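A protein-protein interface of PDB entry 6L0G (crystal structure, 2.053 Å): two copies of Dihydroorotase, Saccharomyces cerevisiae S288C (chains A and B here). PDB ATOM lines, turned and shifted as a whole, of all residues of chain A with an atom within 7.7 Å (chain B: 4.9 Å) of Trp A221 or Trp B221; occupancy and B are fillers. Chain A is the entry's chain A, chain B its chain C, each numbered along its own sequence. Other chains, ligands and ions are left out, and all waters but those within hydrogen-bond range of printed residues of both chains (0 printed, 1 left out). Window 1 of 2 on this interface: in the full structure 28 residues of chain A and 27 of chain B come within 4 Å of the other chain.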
ATOM      1  N   VAL A 153       9.475  23.789 -18.736  1.00  0.00           N
ATOM      2  CA  VAL A 153      10.596  23.136 -18.070  1.00  0.00           C
ATOM      3  C   VAL A 153      10.242  21.728 -17.599  1.00  0.00           C
ATOM      4  O   VAL A 153      11.137  20.910 -17.422  1.00  0.00           O
ATOM      5  CB  VAL A 153      11.117  24.018 -16.909  1.00  0.00           C
ATOM      6  CG1 VAL A 153      11.696  25.311 -17.462  1.00  0.00           C
ATOM      7  CG2 VAL A 153      10.005  24.316 -15.902  1.00  0.00           C
ATOM      8  N   LEU A 154       8.955  21.408 -17.415  1.00  0.00           N
ATOM      9  CA  LEU A 154       8.586  20.072 -16.940  1.00  0.00           C
ATOM     10  C   LEU A 154       8.471  19.026 -18.042  1.00  0.00           C
ATOM     11  O   LEU A 154       8.749  17.845 -17.792  1.00  0.00           O
ATOM     12  CB  LEU A 154       7.257  20.114 -16.201  1.00  0.00           C
ATOM     13  CG  LEU A 154       7.367  19.920 -14.707  1.00  0.00           C
ATOM     14  CD1 LEU A 154       8.290  20.958 -14.133  1.00  0.00           C
ATOM     15  CD2 LEU A 154       5.975  20.076 -14.160  1.00  0.00           C
ATOM     16  N   HIS A 213      20.160  14.893  -9.158  1.00  0.00           N
ATOM     17  CA  HIS A 213      18.848  14.369  -9.522  1.00  0.00           C
ATOM     18  C   HIS A 213      18.497  13.069  -8.806  1.00  0.00           C
ATOM     19  O   HIS A 213      17.350  12.626  -8.911  1.00  0.00           O
ATOM     20  CB  HIS A 213      18.741  14.189 -11.030  1.00  0.00           C
ATOM     21  CG  HIS A 213      18.694  15.489 -11.776  1.00  0.00           C
ATOM     22  ND1 HIS A 213      19.716  15.908 -12.601  1.00  0.00           N
ATOM     23  CD2 HIS A 213      17.761  16.473 -11.800  1.00  0.00           C
ATOM     24  CE1 HIS A 213      19.407  17.089 -13.111  1.00  0.00           C
ATOM     25  NE2 HIS A 213      18.221  17.447 -12.650  1.00  0.00           N
ATOM     26  N   LEU A 216      17.034  15.318  -5.515  1.00  0.00           N
ATOM     27  CA  LEU A 216      16.173  16.494  -5.615  1.00  0.00           C
ATOM     28  C   LEU A 216      14.843  16.186  -6.285  1.00  0.00           C
ATOM     29  O   LEU A 216      14.747  15.286  -7.125  1.00  0.00           O
ATOM     30  CB  LEU A 216      16.869  17.603  -6.408  1.00  0.00           C
ATOM     31  CG  LEU A 216      18.106  18.282  -5.824  1.00  0.00           C
ATOM     32  CD1 LEU A 216      18.623  19.348  -6.785  1.00  0.00           C
ATOM     33  CD2 LEU A 216      17.825  18.875  -4.445  1.00  0.00           C
ATOM     34  N   THR A 217      13.808  16.939  -5.881  1.00  0.00           N
ATOM     35  CA  THR A 217      12.557  17.081  -6.624  1.00  0.00           C
ATOM     36  C   THR A 217      12.236  18.564  -6.748  1.00  0.00           C
ATOM     37  O   THR A 217      12.891  19.420  -6.151  1.00  0.00           O
ATOM     38  CB  THR A 217      11.345  16.386  -5.981  1.00  0.00           C
ATOM     39  OG1 THR A 217      11.014  17.052  -4.760  1.00  0.00           O
ATOM     40  CG2 THR A 217      11.590  14.905  -5.731  1.00  0.00           C
ATOM     41  N   ILE A 218      11.194  18.866  -7.523  1.00  0.00           N
ATOM     42  CA  ILE A 218      10.792  20.258  -7.727  1.00  0.00           C
ATOM     43  C   ILE A 218      10.629  20.987  -6.392  1.00  0.00           C
ATOM     44  O   ILE A 218      10.951  22.177  -6.277  1.00  0.00           O
ATOM     45  CB  ILE A 218       9.505  20.318  -8.569  1.00  0.00           C
ATOM     46  CG1 ILE A 218       9.042  21.767  -8.761  1.00  0.00           C
ATOM     47  CG2 ILE A 218       8.394  19.486  -7.928  1.00  0.00           C
ATOM     48  CD1 ILE A 218       7.992  21.914  -9.830  1.00  0.00           C
ATOM     49  N   ASP A 219      10.156  20.284  -5.355  1.00  0.00           N
ATOM     50  CA  ASP A 219       9.991  20.921  -4.047  1.00  0.00           C
ATOM     51  C   ASP A 219      11.302  21.485  -3.515  1.00  0.00           C
ATOM     52  O   ASP A 219      11.293  22.467  -2.771  1.00  0.00           O
ATOM     53  CB  ASP A 219       9.432  19.921  -3.043  1.00  0.00           C
ATOM     54  CG  ASP A 219       7.949  19.733  -3.182  1.00  0.00           C
ATOM     55  OD1 ASP A 219       7.300  19.421  -2.169  1.00  0.00           O
ATOM     56  OD2 ASP A 219       7.430  19.898  -4.300  1.00  0.00           O
ATOM     57  N   ASP A 220      12.432  20.878  -3.870  1.00  0.00           N
ATOM     58  CA  ASP A 220      13.720  21.317  -3.343  1.00  0.00           C
ATOM     59  C   ASP A 220      14.277  22.569  -4.018  1.00  0.00           C
ATOM     60  O   ASP A 220      15.108  23.252  -3.412  1.00  0.00           O
ATOM     61  CB  ASP A 220      14.724  20.170  -3.441  1.00  0.00           C
ATOM     62  CG  ASP A 220      14.272  18.939  -2.660  1.00  0.00           C
ATOM     63  OD1 ASP A 220      13.957  19.108  -1.477  1.00  0.00           O
ATOM     64  OD2 ASP A 220      14.214  17.814  -3.219  1.00  0.00           O
ATOM     65  N   TRP A 221      13.888  22.877  -5.260  1.00  0.00           N
ATOM     66  CA  TRP A 221      14.402  24.075  -5.913  1.00  0.00           C
ATOM     67  C   TRP A 221      13.351  25.163  -6.078  1.00  0.00           C
ATOM     68  O   TRP A 221      13.716  26.292  -6.423  1.00  0.00           O
ATOM     69  CB  TRP A 221      15.031  23.754  -7.289  1.00  0.00           C
ATOM     70  CG  TRP A 221      14.123  23.137  -8.315  1.00  0.00           C
ATOM     71  CD1 TRP A 221      14.003  21.815  -8.602  1.00  0.00           C
ATOM     72  CD2 TRP A 221      13.235  23.823  -9.208  1.00  0.00           C
ATOM     73  NE1 TRP A 221      13.076  21.620  -9.601  1.00  0.00           N
ATOM     74  CE2 TRP A 221      12.594  22.842  -9.996  1.00  0.00           C
ATOM     75  CE3 TRP A 221      12.918  25.167  -9.419  1.00  0.00           C
ATOM     76  CZ2 TRP A 221      11.646  23.162 -10.965  1.00  0.00           C
ATOM     77  CZ3 TRP A 221      11.976  25.483 -10.379  1.00  0.00           C
ATOM     78  CH2 TRP A 221      11.357  24.487 -11.147  1.00  0.00           C
ATOM     79  N   ALA A 222      12.082  24.885  -5.757  1.00  0.00           N
ATOM     80  CA  ALA A 222      11.034  25.893  -5.913  1.00  0.00           C
ATOM     81  C   ALA A 222      11.403  27.205  -5.222  1.00  0.00           C
ATOM     82  O   ALA A 222      11.348  28.276  -5.831  1.00  0.00           O
ATOM     83  CB  ALA A 222       9.712  25.345  -5.381  1.00  0.00           C
ATOM     84  N   GLY A 223      11.808  27.143  -3.958  1.00  0.00           N
ATOM     85  CA  GLY A 223      12.220  28.327  -3.233  1.00  0.00           C
ATOM     86  C   GLY A 223      13.710  28.419  -2.995  1.00  0.00           C
ATOM     87  O   GLY A 223      14.149  29.301  -2.244  1.00  0.00           O
ATOM     88  N   ASN A 224      14.507  27.533  -3.594  1.00  0.00           N
ATOM     89  CA  ASN A 224      15.931  27.404  -3.303  1.00  0.00           C
ATOM     90  C   ASN A 224      16.721  27.432  -4.601  1.00  0.00           C
ATOM     91  O   ASN A 224      16.959  26.384  -5.222  1.00  0.00           O
ATOM     92  CB  ASN A 224      16.211  26.118  -2.528  1.00  0.00           C
ATOM     93  CG  ASN A 224      15.491  26.069  -1.203  1.00  0.00           C
ATOM     94  OD1 ASN A 224      15.624  26.970  -0.387  1.00  0.00           O
ATOM     95  ND2 ASN A 224      14.741  25.004  -0.976  1.00  0.00           N
ATOM     96  N   PRO A 225      17.116  28.623  -5.054  1.00  0.00           N
ATOM     97  CA  PRO A 225      17.916  28.746  -6.284  1.00  0.00           C
ATOM     98  C   PRO A 225      19.185  27.905  -6.330  1.00  0.00           C
ATOM     99  O   PRO A 225      19.576  27.496  -7.429  1.00  0.00           O
ATOM    100  CB  PRO A 225      18.253  30.239  -6.308  1.00  0.00           C
ATOM    101  CG  PRO A 225      17.101  30.878  -5.587  1.00  0.00           C
ATOM    102  CD  PRO A 225      16.724  29.931  -4.512  1.00  0.00           C
ATOM    103  N   VAL A 226      19.833  27.621  -5.191  1.00  0.00           N
ATOM    104  CA  VAL A 226      21.030  26.773  -5.219  1.00  0.00           C
ATOM    105  C   VAL A 226      20.712  25.409  -5.805  1.00  0.00           C
ATOM    106  O   VAL A 226      21.589  24.766  -6.392  1.00  0.00           O
ATOM    107  CB  VAL A 226      21.639  26.578  -3.812  1.00  0.00           C
ATOM    108  CG1 VAL A 226      22.487  27.744  -3.409  1.00  0.00           C
ATOM    109  CG2 VAL A 226      20.549  26.267  -2.777  1.00  0.00           C
ATOM    110  N   ASN A 227      19.470  24.947  -5.677  1.00  0.00           N
ATOM    111  CA  ASN A 227      19.105  23.647  -6.225  1.00  0.00           C
ATOM    112  C   ASN A 227      18.497  23.731  -7.619  1.00  0.00           C
ATOM    113  O   ASN A 227      18.076  22.696  -8.152  1.00  0.00           O
ATOM    114  CB  ASN A 227      18.124  22.934  -5.285  1.00  0.00           C
ATOM    115  CG  ASN A 227      18.793  22.459  -4.012  1.00  0.00           C
ATOM    116  OD1 ASN A 227      20.013  22.214  -3.997  1.00  0.00           O
ATOM    117  ND2 ASN A 227      18.016  22.343  -2.936  1.00  0.00           N
ATOM    118  N   PHE A 228      18.451  24.922  -8.215  1.00  0.00           N
ATOM    119  CA  PHE A 228      17.881  25.101  -9.547  1.00  0.00           C
ATOM    120  C   PHE A 228      18.938  24.773 -10.579  1.00  0.00           C
ATOM    121  O   PHE A 228      20.038  25.331 -10.552  1.00  0.00           O
ATOM    122  CB  PHE A 228      17.369  26.527  -9.752  1.00  0.00           C
ATOM    123  CG  PHE A 228      16.934  26.824 -11.173  1.00  0.00           C
ATOM    124  CD1 PHE A 228      15.841  26.175 -11.738  1.00  0.00           C
ATOM    125  CD2 PHE A 228      17.609  27.766 -11.939  1.00  0.00           C
ATOM    126  CE1 PHE A 228      15.425  26.453 -13.038  1.00  0.00           C
ATOM    127  CE2 PHE A 228      17.189  28.043 -13.258  1.00  0.00           C
ATOM    128  CZ  PHE A 228      16.100  27.378 -13.795  1.00  0.00           C
ATOM    129  N   CYS A 229      18.614  23.849 -11.469  1.00  0.00           N
ATOM    130  CA  CYS A 229      19.518  23.460 -12.531  1.00  0.00           C
ATOM    131  C   CYS A 229      18.665  23.107 -13.742  1.00  0.00           C
ATOM    132  O   CYS A 229      17.440  22.995 -13.643  1.00  0.00           O
ATOM    133  CB  CYS A 229      20.400  22.279 -12.087  1.00  0.00           C
ATOM    134  SG  CYS A 229      19.452  20.740 -11.845  1.00  0.00           S
ATOM    135  N   PRO A 231      18.416  19.981 -16.799  1.00  0.00           N
ATOM    136  CA  PRO A 231      16.949  20.010 -16.693  1.00  0.00           C
ATOM    137  C   PRO A 231      16.514  20.058 -15.221  1.00  0.00           C
ATOM    138  O   PRO A 231      17.254  19.569 -14.353  1.00  0.00           O
ATOM    139  CB  PRO A 231      16.506  18.692 -17.366  1.00  0.00           C
ATOM    140  CG  PRO A 231      17.786  18.105 -18.011  1.00  0.00           C
ATOM    141  CD  PRO A 231      18.892  18.630 -17.140  1.00  0.00           C
ATOM    142  N   VAL A 232      15.369  20.686 -14.938  1.00  0.00           N
ATOM    143  CA  VAL A 232      14.918  20.844 -13.556  1.00  0.00           C
ATOM    144  C   VAL A 232      14.608  19.485 -12.942  1.00  0.00           C
ATOM    145  O   VAL A 232      14.158  18.558 -13.626  1.00  0.00           O
ATOM    146  CB  VAL A 232      13.688  21.767 -13.492  1.00  0.00           C
ATOM    147  CG1 VAL A 232      14.008  23.132 -14.113  1.00  0.00           C
ATOM    148  CG2 VAL A 232      12.490  21.110 -14.168  1.00  0.00           C
ATOM    149  N   ALA A 233      14.868  19.350 -11.640  1.00  0.00           N
ATOM    150  CA  ALA A 233      14.378  18.175 -10.921  1.00  0.00           C
ATOM    151  C   ALA A 233      12.847  18.148 -10.945  1.00  0.00           C
ATOM    152  O   ALA A 233      12.191  19.184 -10.799  1.00  0.00           O
ATOM    153  CB  ALA A 233      14.897  18.169  -9.483  1.00  0.00           C
ATOM    154  N   LYS A 234      12.270  16.975 -11.161  1.00  0.00           N
ATOM    155  CA  LYS A 234      10.850  16.857 -11.488  1.00  0.00           C
ATOM    156  C   LYS A 234      10.111  16.199 -10.327  1.00  0.00           C
ATOM    157  O   LYS A 234      10.296  16.638  -9.189  1.00  0.00           O
ATOM    158  CB  LYS A 234      10.710  16.173 -12.838  1.00  0.00           C
ATOM    159  CG  LYS A 234      11.230  17.082 -13.969  1.00  0.00           C
ATOM    160  CD  LYS A 234      11.329  16.372 -15.299  1.00  0.00           C
ATOM    161  CE  LYS A 234      11.726  17.355 -16.402  1.00  0.00           C
ATOM    162  NZ  LYS A 234      13.153  17.792 -16.319  1.00  0.00           N
ATOM    163  N   LEU A 235       9.264  15.230 -10.553  1.00  0.00           N
ATOM    164  CA  LEU A 235       8.369  14.761  -9.508  1.00  0.00           C
ATOM    165  C   LEU A 235       8.959  13.561  -8.773  1.00  0.00           C
ATOM    166  O   LEU A 235       9.896  12.917  -9.267  1.00  0.00           O
ATOM    167  CB  LEU A 235       7.019  14.405 -10.117  1.00  0.00           C
ATOM    168  CG  LEU A 235       6.448  15.487 -11.030  1.00  0.00           C
ATOM    169  CD1 LEU A 235       5.131  15.018 -11.650  1.00  0.00           C
ATOM    170  CD2 LEU A 235       6.245  16.789 -10.264  1.00  0.00           C
ATOM    171  N   TYR A 270      16.836  38.029  -7.926  1.00  0.00           N
ATOM    172  CA  TYR A 270      15.384  37.894  -8.003  1.00  0.00           C
ATOM    173  C   TYR A 270      14.916  37.479  -9.390  1.00  0.00           C
ATOM    174  O   TYR A 270      13.771  37.050  -9.530  1.00  0.00           O
ATOM    175  CB  TYR A 270      14.663  39.173  -7.547  1.00  0.00           C
ATOM    176  CG  TYR A 270      14.867  40.424  -8.380  1.00  0.00           C
ATOM    177  CD1 TYR A 270      15.708  41.438  -7.933  1.00  0.00           C
ATOM    178  CD2 TYR A 270      14.184  40.615  -9.578  1.00  0.00           C
ATOM    179  CE1 TYR A 270      15.882  42.596  -8.661  1.00  0.00           C
ATOM    180  CE2 TYR A 270      14.356  41.783 -10.323  1.00  0.00           C
ATOM    181  CZ  TYR A 270      15.210  42.761  -9.850  1.00  0.00           C
ATOM    182  OH  TYR A 270      15.396  43.911 -10.563  1.00  0.00           O
ATOM    183  N   VAL A 273      18.319  33.690 -12.223  1.00  0.00           N
ATOM    184  CA  VAL A 273      19.172  32.800 -11.443  1.00  0.00           C
ATOM    185  C   VAL A 273      19.901  31.856 -12.389  1.00  0.00           C
ATOM    186  O   VAL A 273      19.275  31.185 -13.217  1.00  0.00           O
ATOM    187  CB  VAL A 273      18.332  31.995 -10.433  1.00  0.00           C
ATOM    188  CG1 VAL A 273      19.107  30.773  -9.962  1.00  0.00           C
ATOM    189  CG2 VAL A 273      17.904  32.863  -9.230  1.00  0.00           C
ATOM    190  N   VAL A 277      24.081  23.031 -10.351  1.00  0.00           N
ATOM    191  CA  VAL A 277      24.365  22.543  -9.011  1.00  0.00           C
ATOM    192  C   VAL A 277      25.841  22.173  -8.987  1.00  0.00           C
ATOM    193  O   VAL A 277      26.321  21.483  -9.893  1.00  0.00           O
ATOM    194  CB  VAL A 277      23.482  21.329  -8.657  1.00  0.00           C
ATOM    195  CG1 VAL A 277      23.885  20.725  -7.315  1.00  0.00           C
ATOM    196  CG2 VAL A 277      22.007  21.720  -8.640  1.00  0.00           C
ATOM    197  N   THR B 217       2.983  30.846 -15.756  1.00  0.00           N
ATOM    198  CA  THR B 217       3.116  29.398 -15.738  1.00  0.00           C
ATOM    199  C   THR B 217       4.469  29.057 -15.115  1.00  0.00           C
ATOM    200  O   THR B 217       5.264  29.939 -14.759  1.00  0.00           O
ATOM    201  CB  THR B 217       2.986  28.766 -17.132  1.00  0.00           C
ATOM    202  OG1 THR B 217       4.065  29.217 -17.947  1.00  0.00           O
ATOM    203  CG2 THR B 217       1.653  29.160 -17.791  1.00  0.00           C
ATOM    204  N   ILE B 218       4.706  27.758 -14.945  1.00  0.00           N
ATOM    205  CA  ILE B 218       5.928  27.300 -14.296  1.00  0.00           C
ATOM    206  C   ILE B 218       7.168  27.922 -14.933  1.00  0.00           C
ATOM    207  O   ILE B 218       8.103  28.313 -14.232  1.00  0.00           O
ATOM    208  CB  ILE B 218       5.987  25.760 -14.301  1.00  0.00           C
ATOM    209  CG1 ILE B 218       7.218  25.285 -13.532  1.00  0.00           C
ATOM    210  CG2 ILE B 218       5.963  25.221 -15.732  1.00  0.00           C
ATOM    211  CD1 ILE B 218       7.028  23.967 -12.845  1.00  0.00           C
ATOM    212  N   ASP B 219       7.172  28.092 -16.254  1.00  0.00           N
ATOM    213  CA  ASP B 219       8.342  28.679 -16.906  1.00  0.00           C
ATOM    214  C   ASP B 219       8.639  30.099 -16.435  1.00  0.00           C
ATOM    215  O   ASP B 219       9.795  30.523 -16.465  1.00  0.00           O
ATOM    216  CB  ASP B 219       8.164  28.665 -18.412  1.00  0.00           C
ATOM    217  CG  ASP B 219       8.622  27.370 -19.032  1.00  0.00           C
ATOM    218  OD1 ASP B 219       8.682  26.343 -18.325  1.00  0.00           O
ATOM    219  OD2 ASP B 219       8.925  27.383 -20.235  1.00  0.00           O
ATOM    220  N   ASP B 220       7.627  30.854 -16.007  1.00  0.00           N
ATOM    221  CA  ASP B 220       7.896  32.229 -15.603  1.00  0.00           C
ATOM    222  C   ASP B 220       8.622  32.318 -14.271  1.00  0.00           C
ATOM    223  O   ASP B 220       9.251  33.350 -14.000  1.00  0.00           O
ATOM    224  CB  ASP B 220       6.602  33.033 -15.522  1.00  0.00           C
ATOM    225  CG  ASP B 220       5.880  33.092 -16.834  1.00  0.00           C
ATOM    226  OD1 ASP B 220       6.448  33.649 -17.788  1.00  0.00           O
ATOM    227  OD2 ASP B 220       4.745  32.568 -16.916  1.00  0.00           O
ATOM    228  N   TRP B 221       8.526  31.295 -13.410  1.00  0.00           N
ATOM    229  CA  TRP B 221       9.228  31.356 -12.141  1.00  0.00           C
ATOM    230  C   TRP B 221      10.397  30.378 -12.045  1.00  0.00           C
ATOM    231  O   TRP B 221      11.152  30.452 -11.070  1.00  0.00           O
ATOM    232  CB  TRP B 221       8.261  31.156 -10.954  1.00  0.00           C
ATOM    233  CG  TRP B 221       7.483  29.862 -10.886  1.00  0.00           C
ATOM    234  CD1 TRP B 221       6.242  29.621 -11.414  1.00  0.00           C
ATOM    235  CD2 TRP B 221       7.875  28.647 -10.226  1.00  0.00           C
ATOM    236  NE1 TRP B 221       5.844  28.332 -11.134  1.00  0.00           N
ATOM    237  CE2 TRP B 221       6.830  27.714 -10.410  1.00  0.00           C
ATOM    238  CE3 TRP B 221       9.009  28.257  -9.501  1.00  0.00           C
ATOM    239  CZ2 TRP B 221       6.894  26.418  -9.906  1.00  0.00           C
ATOM    240  CZ3 TRP B 221       9.074  26.978  -9.008  1.00  0.00           C
ATOM    241  CH2 TRP B 221       8.022  26.069  -9.204  1.00  0.00           C
ATOM    242  N   ALA B 222      10.546  29.447 -12.995  1.00  0.00           N
ATOM    243  CA  ALA B 222      11.735  28.605 -13.048  1.00  0.00           C
ATOM    244  C   ALA B 222      12.943  29.494 -13.313  1.00  0.00           C
ATOM    245  O   ALA B 222      13.198  29.879 -14.456  1.00  0.00           O
ATOM    246  CB  ALA B 222      11.585  27.513 -14.109  1.00  0.00           C
ATOM    247  N   GLY B 223      13.677  29.843 -12.278  1.00  0.00           N
ATOM    248  CA  GLY B 223      14.810  30.732 -12.406  1.00  0.00           C
ATOM    249  C   GLY B 223      14.511  32.185 -12.086  1.00  0.00           C
ATOM    250  O   GLY B 223      15.437  33.010 -12.127  1.00  0.00           O
ATOM    251  N   ASN B 224      13.271  32.520 -11.705  1.00  0.00           N
ATOM    252  CA  ASN B 224      12.912  33.903 -11.382  1.00  0.00           C
ATOM    253  C   ASN B 224      12.152  33.911 -10.065  1.00  0.00           C
ATOM    254  O   ASN B 224      10.910  33.909 -10.051  1.00  0.00           O
ATOM    255  CB  ASN B 224      12.078  34.566 -12.479  1.00  0.00           C
ATOM    256  CG  ASN B 224      12.736  34.491 -13.848  1.00  0.00           C
ATOM    257  OD1 ASN B 224      13.914  34.842 -14.014  1.00  0.00           O
ATOM    258  ND2 ASN B 224      11.970  34.048 -14.845  1.00  0.00           N
ATOM    259  N   PRO B 225      12.861  33.953  -8.945  1.00  0.00           N
ATOM    260  CA  PRO B 225      12.183  34.025  -7.645  1.00  0.00           C
ATOM    261  C   PRO B 225      11.133  35.133  -7.550  1.00  0.00           C
ATOM    262  O   PRO B 225      10.171  34.979  -6.785  1.00  0.00           O
ATOM    263  CB  PRO B 225      13.344  34.261  -6.673  1.00  0.00           C
ATOM    264  CG  PRO B 225      14.514  33.568  -7.320  1.00  0.00           C
ATOM    265  CD  PRO B 225      14.324  33.781  -8.802  1.00  0.00           C
ATOM    266  N   ASN B 227       8.810  35.775  -9.488  1.00  0.00           N
ATOM    267  CA  ASN B 227       7.521  35.212  -9.863  1.00  0.00           C
ATOM    268  C   ASN B 227       7.119  33.995  -9.039  1.00  0.00           C
ATOM    269  O   ASN B 227       6.094  33.360  -9.350  1.00  0.00           O
ATOM    270  CB  ASN B 227       7.539  34.862 -11.338  1.00  0.00           C
ATOM    271  CG  ASN B 227       7.510  36.092 -12.192  1.00  0.00           C
ATOM    272  OD1 ASN B 227       6.906  37.105 -11.808  1.00  0.00           O
ATOM    273  ND2 ASN B 227       8.189  36.039 -13.336  1.00  0.00           N
ATOM    274  N   PHE B 228       7.908  33.652  -8.017  1.00  0.00           N
ATOM    275  CA  PHE B 228       7.653  32.497  -7.168  1.00  0.00           C
ATOM    276  C   PHE B 228       6.675  32.889  -6.076  1.00  0.00           C
ATOM    277  O   PHE B 228       6.922  33.842  -5.324  1.00  0.00           O
ATOM    278  CB  PHE B 228       8.963  31.973  -6.563  1.00  0.00           C
ATOM    279  CG  PHE B 228       8.768  30.938  -5.473  1.00  0.00           C
ATOM    280  CD1 PHE B 228       8.198  29.721  -5.753  1.00  0.00           C
ATOM    281  CD2 PHE B 228       9.168  31.195  -4.172  1.00  0.00           C
ATOM    282  CE1 PHE B 228       8.009  28.749  -4.743  1.00  0.00           C
ATOM    283  CE2 PHE B 228       8.998  30.247  -3.154  1.00  0.00           C
ATOM    284  CZ  PHE B 228       8.406  29.016  -3.441  1.00  0.00           C
ATOM    285  N   VAL B 232       2.081  27.572  -6.258  1.00  0.00           N
ATOM    286  CA  VAL B 232       2.943  27.840  -7.394  1.00  0.00           C
ATOM    287  C   VAL B 232       2.104  27.906  -8.669  1.00  0.00           C
ATOM    288  O   VAL B 232       1.127  27.159  -8.821  1.00  0.00           O
ATOM    289  CB  VAL B 232       3.975  26.700  -7.387  1.00  0.00           C
ATOM    290  CG1 VAL B 232       3.887  25.834  -8.590  1.00  0.00           C
ATOM    291  CG2 VAL B 232       5.342  27.168  -6.967  1.00  0.00           C
ATOM    292  N   ALA B 233       2.458  28.814  -9.583  1.00  0.00           N
ATOM    293  CA  ALA B 233       1.865  28.778 -10.922  1.00  0.00           C
ATOM    294  C   ALA B 233       2.237  27.480 -11.638  1.00  0.00           C
ATOM    295  O   ALA B 233       3.388  27.037 -11.596  1.00  0.00           O
ATOM    296  CB  ALA B 233       2.315  29.979 -11.761  1.00  0.00           C
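N of Val A273 sits at hydrogen-bond distance from O of Gly B223 (3.0 Å). O of Tyr A270 sits close to N of Pro B225, at 3.3 Å. The backbone NH (N) of Val A153 sits at hydrogen-bond distance from the side-chain carboxylate (OD1) of Asp B219.
NE1 of Trp B221 sits at hydrogen-bond distance from O of Ala B233, 2.8 Å away. N of Ile A218 is in hydrogen-bond range of O of Ala A233 (3.4 Å). The indole nitrogen (NE1) of Trp A221 is in hydrogen-bond range of the backbone carbonyl oxygen (O) of Ala A233. O of Asp B220 sits at hydrogen-bond distance from ND2 of Asn B224 (2.9 Å). The backbone NH of Ile A218 lies within hydrogen-bond range of the backbone carbonyl oxygen of Lys A234 (2.9 Å).
Ala B222 touches Val A153 (CB to CG2, 3.99 Å). Leu A154 touches Ile B218. CD1 of Ile A218 touches CD1 of Ile B218, 3.8 Å away. Trp A221 touches Trp B221 (CZ3 to CZ3, 3.5 Å). Trp B221 touches Ala A222 (CZ3 to CA, 3.8 Å). O of Ala A222 touches CD1 of Phe B228, at 3.5 Å. Gly A223 touches Phe B228 (CA to CE2, 3.8 Å). Phe A228 touches Ala B222 (CZ to C, 3.8 Å). Asn B224 touches Tyr A270 (C to O, 3.6 Å). CD of Pro B225 touches CG2 of Val A273 (3.7 Å).
Of the printed residues of chain B, Trp A221 touches Trp B221 (3.5 Å). Of chain A, only Trp A221 and Ala A222 come within 4 Å of Trp B221. Of the printed residues of chain A, Asn B224 touches Tyr A270. Printed residues of chain B within 4 Å of Val A153: Ile B218 (3.8 Å), Asp B219 (2.7 Å) and Ala B222 (3.99 Å). Of the printed residues of chain A, Ile B218 touches Val A153 (3.8 Å), Leu A154 (3.5 Å) and Ile A218 (3.8 Å). Printed residues of chain A within 4 Å of Phe B228: Ala A222 (3.5 Å) and Gly A223 (3.8 Å). Asp B220 touches none of the printed residues of chain A. The nearest residue of chain A that does not touch Trp B221 is Ile A218 (4.2 Å). The nearest printed residue of chain B that does not touch Leu A154 is Asp B219 (5.0 Å).
Of the 25 printed residues of chain A, 9 touch a printed residue of chain B. Hydrophobic or aromatic side chains of chain A that line the printed part of chain B: Val A153, Leu A154, Ile A218, Trp A221, Ala A222, Phe A228 and Val A273. Of the 13 printed residues of chain B, 8 touch a printed residue of chain A. Hydrophobic or aromatic side chains of chain B within 4 Å of the printed part of chain A: Ile B218, Trp B221, Ala B222, Pro B225 and Phe B228. Among the printed residues, 15 pairs touch across the chains.
Ile A218 touches its own counterpart, Ile B218. Trp A221 touches its own counterpart, Trp B221. Ala A222 touches Trp B221, but with the chains exchanged Trp A221 does not touch Ala B222 (4.1 Å). Gly A223 touches Phe B228, and with the chains exchanged Phe A228 touches Gly B223. Positions printed for both chains: 217, 218, 219, 220, 221, 222, 223, 224, 225, 227, 228, 232 and 233. Of the 15 pairs that touch across the chains among the printed residues, 6 have their exchanged pair printed and touching as well.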
